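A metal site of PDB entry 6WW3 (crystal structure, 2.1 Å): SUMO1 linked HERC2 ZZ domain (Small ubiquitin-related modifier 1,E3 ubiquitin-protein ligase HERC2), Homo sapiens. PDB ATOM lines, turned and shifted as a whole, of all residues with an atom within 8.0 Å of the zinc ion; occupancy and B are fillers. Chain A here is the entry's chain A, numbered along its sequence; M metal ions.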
ATOM      1  N   LYS A  27     -18.083 -18.237  31.138  1.00  0.00           N
ATOM      2  CA  LYS A  27     -16.756 -18.822  30.982  1.00  0.00           C
ATOM      3  C   LYS A  27     -16.034 -18.158  29.813  1.00  0.00           C
ATOM      4  O   LYS A  27     -16.567 -18.083  28.704  1.00  0.00           O
ATOM      5  CB  LYS A  27     -16.842 -20.329  30.752  1.00  0.00           C
ATOM      6  CG  LYS A  27     -15.456 -20.977  30.531  1.00  0.00           C
ATOM      7  CD  LYS A  27     -15.532 -22.504  30.443  1.00  0.00           C
ATOM      8  CE  LYS A  27     -14.190 -23.143  30.087  1.00  0.00           C
ATOM      9  NZ  LYS A  27     -13.058 -22.740  30.976  1.00  0.00           N
ATOM     10  N   CYS A  28     -14.824 -17.675  30.059  1.00  0.00           N
ATOM     11  CA  CYS A  28     -14.050 -17.082  28.974  1.00  0.00           C
ATOM     12  C   CYS A  28     -13.625 -18.158  27.992  1.00  0.00           C
ATOM     13  O   CYS A  28     -13.121 -19.213  28.395  1.00  0.00           O
ATOM     14  CB  CYS A  28     -12.821 -16.354  29.498  1.00  0.00           C
ATOM     15  SG  CYS A  28     -11.959 -15.503  28.167  1.00  0.00           S
ATOM     16  N   ARG A  29     -13.814 -17.895  26.690  1.00  0.00           N
ATOM     17  CA  ARG A  29     -13.409 -18.838  25.647  1.00  0.00           C
ATOM     18  C   ARG A  29     -11.929 -18.784  25.309  1.00  0.00           C
ATOM     19  O   ARG A  29     -11.433 -19.664  24.609  1.00  0.00           O
ATOM     20  CB  ARG A  29     -14.220 -18.604  24.361  1.00  0.00           C
ATOM     21  CG  ARG A  29     -15.725 -18.847  24.522  1.00  0.00           C
ATOM     22  CD  ARG A  29     -16.523 -18.526  23.259  1.00  0.00           C
ATOM     23  NE  ARG A  29     -17.826 -19.203  23.282  1.00  0.00           N
ATOM     24  CZ  ARG A  29     -19.008 -18.595  23.262  1.00  0.00           C
ATOM     25  NH1 ARG A  29     -20.125 -19.321  23.292  1.00  0.00           N
ATOM     26  NH2 ARG A  29     -19.087 -17.276  23.209  1.00  0.00           N
ATOM     27  N   ASN A  30     -11.198 -17.803  25.837  1.00  0.00           N
ATOM     28  CA  ASN A  30      -9.803 -17.584  25.463  1.00  0.00           C
ATOM     29  C   ASN A  30      -8.846 -17.873  26.602  1.00  0.00           C
ATOM     30  O   ASN A  30      -7.844 -18.564  26.411  1.00  0.00           O
ATOM     31  CB  ASN A  30      -9.662 -16.137  24.994  1.00  0.00           C
ATOM     32  CG  ASN A  30     -10.738 -15.774  23.984  1.00  0.00           C
ATOM     33  OD1 ASN A  30     -11.872 -15.439  24.366  1.00  0.00           O
ATOM     34  ND2 ASN A  30     -10.376 -15.792  22.704  1.00  0.00           N
ATOM     35  N   CYS A  31      -9.136 -17.378  27.809  1.00  0.00           N
ATOM     36  CA  CYS A  31      -8.415 -17.796  28.992  1.00  0.00           C
ATOM     37  C   CYS A  31      -8.531 -19.309  29.181  1.00  0.00           C
ATOM     38  O   CYS A  31      -9.457 -19.962  28.680  1.00  0.00           O
ATOM     39  CB  CYS A  31      -8.938 -17.072  30.239  1.00  0.00           C
ATOM     40  SG  CYS A  31      -8.680 -15.288  30.291  1.00  0.00           S
ATOM     41  N   ASP A  32      -7.545 -19.864  29.895  1.00  0.00           N
ATOM     42  CA  ASP A  32      -7.477 -21.306  30.146  1.00  0.00           C
ATOM     43  C   ASP A  32      -8.597 -21.780  31.076  1.00  0.00           C
ATOM     44  O   ASP A  32      -9.234 -22.805  30.808  1.00  0.00           O
ATOM     45  CB  ASP A  32      -6.096 -21.629  30.735  1.00  0.00           C
ATOM     46  CG  ASP A  32      -5.921 -23.099  31.106  1.00  0.00           C
ATOM     47  OD1 ASP A  32      -5.461 -23.891  30.273  1.00  0.00           O
ATOM     48  OD2 ASP A  32      -6.222 -23.449  32.264  1.00  0.00           O
ATOM     49  N   ASP A  33      -8.875 -21.032  32.148  1.00  0.00           N
ATOM     50  CA  ASP A  33      -9.755 -21.520  33.203  1.00  0.00           C
ATOM     51  C   ASP A  33     -10.338 -20.331  33.951  1.00  0.00           C
ATOM     52  O   ASP A  33     -10.081 -20.161  35.147  1.00  0.00           O
ATOM     53  CB  ASP A  33      -8.966 -22.449  34.131  1.00  0.00           C
ATOM     54  CG  ASP A  33      -9.799 -22.994  35.291  1.00  0.00           C
ATOM     55  OD1 ASP A  33      -9.249 -23.030  36.393  1.00  0.00           O
ATOM     56  OD2 ASP A  33     -10.961 -23.405  35.102  1.00  0.00           O
ATOM     57  N   PHE A  34     -11.099 -19.471  33.265  1.00  0.00           N
ATOM     58  CA  PHE A  34     -11.538 -18.195  33.828  1.00  0.00           C
ATOM     59  C   PHE A  34     -13.042 -18.064  33.715  1.00  0.00           C
ATOM     60  O   PHE A  34     -13.600 -18.209  32.619  1.00  0.00           O
ATOM     61  CB  PHE A  34     -10.842 -17.021  33.119  1.00  0.00           C
ATOM     62  CG  PHE A  34     -11.058 -15.669  33.777  1.00  0.00           C
ATOM     63  CD1 PHE A  34     -12.265 -14.993  33.615  1.00  0.00           C
ATOM     64  CD2 PHE A  34     -10.064 -15.079  34.546  1.00  0.00           C
ATOM     65  CE1 PHE A  34     -12.474 -13.754  34.232  1.00  0.00           C
ATOM     66  CE2 PHE A  34     -10.258 -13.838  35.144  1.00  0.00           C
ATOM     67  CZ  PHE A  34     -11.470 -13.169  34.981  1.00  0.00           C
ATOM     68  N   ASP A  35     -13.697 -17.753  34.830  1.00  0.00           N
ATOM     69  CA  ASP A  35     -15.141 -17.622  34.904  1.00  0.00           C
ATOM     70  C   ASP A  35     -15.526 -16.353  35.643  1.00  0.00           C
ATOM     71  O   ASP A  35     -14.819 -15.913  36.550  1.00  0.00           O
ATOM     72  CB  ASP A  35     -15.796 -18.825  35.597  1.00  0.00           C
ATOM     73  CG  ASP A  35     -15.445 -20.149  34.923  1.00  0.00           C
ATOM     74  OD1 ASP A  35     -14.421 -20.761  35.289  1.00  0.00           O
ATOM     75  OD2 ASP A  35     -16.212 -20.598  34.050  1.00  0.00           O
ATOM     76  N   PHE A  36     -16.658 -15.757  35.236  1.00  0.00           N
ATOM     77  CA  PHE A  36     -17.282 -14.617  35.898  1.00  0.00           C
ATOM     78  C   PHE A  36     -18.678 -14.980  36.349  1.00  0.00           C
ATOM     79  O   PHE A  36     -19.413 -15.639  35.616  1.00  0.00           O
ATOM     80  CB  PHE A  36     -17.423 -13.426  34.931  1.00  0.00           C
ATOM     81  CG  PHE A  36     -16.249 -12.504  34.891  1.00  0.00           C
ATOM     82  CD1 PHE A  36     -15.458 -12.296  36.012  1.00  0.00           C
ATOM     83  CD2 PHE A  36     -15.959 -11.798  33.738  1.00  0.00           C
ATOM     84  CE1 PHE A  36     -14.400 -11.414  35.969  1.00  0.00           C
ATOM     85  CE2 PHE A  36     -14.887 -10.913  33.696  1.00  0.00           C
ATOM     86  CZ  PHE A  36     -14.107 -10.721  34.806  1.00  0.00           C
ATOM     87  N   HIS A  46     -11.789  -6.881  31.513  1.00  0.00           N
ATOM     88  CA  HIS A  46     -11.218  -8.109  30.994  1.00  0.00           C
ATOM     89  C   HIS A  46     -10.788  -7.816  29.577  1.00  0.00           C
ATOM     90  O   HIS A  46     -11.326  -6.901  28.946  1.00  0.00           O
ATOM     91  CB  HIS A  46     -12.226  -9.277  31.038  1.00  0.00           C
ATOM     92  CG  HIS A  46     -11.601 -10.633  30.935  1.00  0.00           C
ATOM     93  ND1 HIS A  46     -11.073 -11.288  32.033  1.00  0.00           N
ATOM     94  CD2 HIS A  46     -11.427 -11.468  29.881  1.00  0.00           C
ATOM     95  CE1 HIS A  46     -10.596 -12.458  31.646  1.00  0.00           C
ATOM     96  NE2 HIS A  46     -10.784 -12.581  30.347  1.00  0.00           N
ATOM     97  N   ASN A  47      -9.825  -8.598  29.078  1.00  0.00           N
ATOM     98  CA  ASN A  47      -9.347  -8.420  27.713  1.00  0.00           C
ATOM     99  C   ASN A  47     -10.534  -8.281  26.778  1.00  0.00           C
ATOM    100  O   ASN A  47     -11.404  -9.156  26.731  1.00  0.00           O
ATOM    101  CB  ASN A  47      -8.476  -9.617  27.307  1.00  0.00           C
ATOM    102  CG  ASN A  47      -7.893  -9.487  25.902  1.00  0.00           C
ATOM    103  OD1 ASN A  47      -8.595  -9.167  24.951  1.00  0.00           O
ATOM    104  ND2 ASN A  47      -6.598  -9.777  25.769  1.00  0.00           N
ATOM    105  N   THR A  48     -10.620  -7.147  26.118  1.00  0.00           N
ATOM    106  CA  THR A  48     -11.766  -6.823  25.282  1.00  0.00           C
ATOM    107  C   THR A  48     -11.900  -7.690  24.054  1.00  0.00           C
ATOM    108  O   THR A  48     -12.895  -7.687  23.468  1.00  0.00           O
ATOM    109  CB  THR A  48     -11.785  -5.330  24.897  1.00  0.00           C
ATOM    110  OG1 THR A  48     -10.575  -4.987  24.265  1.00  0.00           O
ATOM    111  CG2 THR A  48     -11.957  -4.467  26.163  1.00  0.00           C
ATOM    112  N   ARG A  49     -10.876  -8.420  23.713  1.00  0.00           N
ATOM    113  CA  ARG A  49     -10.945  -9.320  22.592  1.00  0.00           C
ATOM    114  C   ARG A  49     -11.304 -10.742  23.050  1.00  0.00           C
ATOM    115  O   ARG A  49     -11.526 -11.559  22.246  1.00  0.00           O
ATOM    116  CB  ARG A  49      -9.716  -9.266  21.715  1.00  0.00           C
ATOM    117  CG  ARG A  49      -9.508  -7.980  20.988  1.00  0.00           C
ATOM    118  CD  ARG A  49     -10.541  -7.703  19.891  1.00  0.00           C
ATOM    119  NE  ARG A  49     -10.672  -6.278  19.785  1.00  0.00           N
ATOM    120  CZ  ARG A  49     -10.003  -5.565  18.903  1.00  0.00           C
ATOM    121  NH1 ARG A  49     -10.155  -4.272  18.913  1.00  0.00           N
ATOM    122  NH2 ARG A  49      -9.165  -6.157  18.023  1.00  0.00           N
ATOM    123  N   HIS A  50     -11.320 -11.014  24.330  1.00  0.00           N
ATOM    124  CA  HIS A  50     -11.839 -12.317  24.763  1.00  0.00           C
ATOM    125  C   HIS A  50     -13.370 -12.291  24.655  1.00  0.00           C
ATOM    126  O   HIS A  50     -13.936 -11.276  24.747  1.00  0.00           O
ATOM    127  CB  HIS A  50     -11.371 -12.746  26.171  1.00  0.00           C
ATOM    128  CG  HIS A  50      -9.901 -12.910  26.239  1.00  0.00           C
ATOM    129  ND1 HIS A  50      -9.267 -13.405  27.331  1.00  0.00           N
ATOM    130  CD2 HIS A  50      -8.939 -12.647  25.349  1.00  0.00           C
ATOM    131  CE1 HIS A  50      -7.973 -13.437  27.113  1.00  0.00           C
ATOM    132  NE2 HIS A  50      -7.764 -13.015  25.906  1.00  0.00           N
ATOM    133  N   THR A  51     -13.997 -13.429  24.457  1.00  0.00           N
ATOM    134  CA  THR A  51     -15.451 -13.577  24.414  1.00  0.00           C
ATOM    135  C   THR A  51     -15.837 -14.648  25.428  1.00  0.00           C
ATOM    136  O   THR A  51     -15.090 -15.602  25.638  1.00  0.00           O
ATOM    137  CB  THR A  51     -15.976 -13.980  23.024  1.00  0.00           C
ATOM    138  OG1 THR A  51     -15.393 -15.228  22.627  1.00  0.00           O
ATOM    139  CG2 THR A  51     -15.638 -12.909  21.984  1.00  0.00           C
ATOM    140  N   PHE A  52     -16.972 -14.451  26.089  1.00  0.00           N
ATOM    141  CA  PHE A  52     -17.454 -15.365  27.107  1.00  0.00           C
ATOM    142  C   PHE A  52     -18.635 -16.192  26.606  1.00  0.00           C
ATOM    143  O   PHE A  52     -19.489 -15.682  25.874  1.00  0.00           O
ATOM    144  CB  PHE A  52     -17.878 -14.576  28.356  1.00  0.00           C
ATOM    145  CG  PHE A  52     -16.737 -14.020  29.139  1.00  0.00           C
ATOM    146  CD1 PHE A  52     -16.039 -12.897  28.690  1.00  0.00           C
ATOM    147  CD2 PHE A  52     -16.352 -14.603  30.333  1.00  0.00           C
ATOM    148  CE1 PHE A  52     -14.991 -12.391  29.412  1.00  0.00           C
ATOM    149  CE2 PHE A  52     -15.293 -14.096  31.077  1.00  0.00           C
ATOM    150  CZ  PHE A  52     -14.613 -12.983  30.616  1.00  0.00           C
HETATM  151 ZN    ZN M   1     -10.284 -14.210  29.110  1.00  0.00          ZN
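The zinc ion is bound by NE2 of His 46, ND1 of His 50, SG of Cys 31 and SG of Cys 28. The zinc ion has four donor atoms within binding distance.
The side-chain amide oxygen (OD1) of Asn 47 sits at hydrogen-bond distance from the backbone NH (N) of His 50. N of Asn 30 sits close to SG of Cys 28 (3.4 Å). N of Cys 28 sits at hydrogen-bond distance from O of Phe 34 (2.9 Å).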
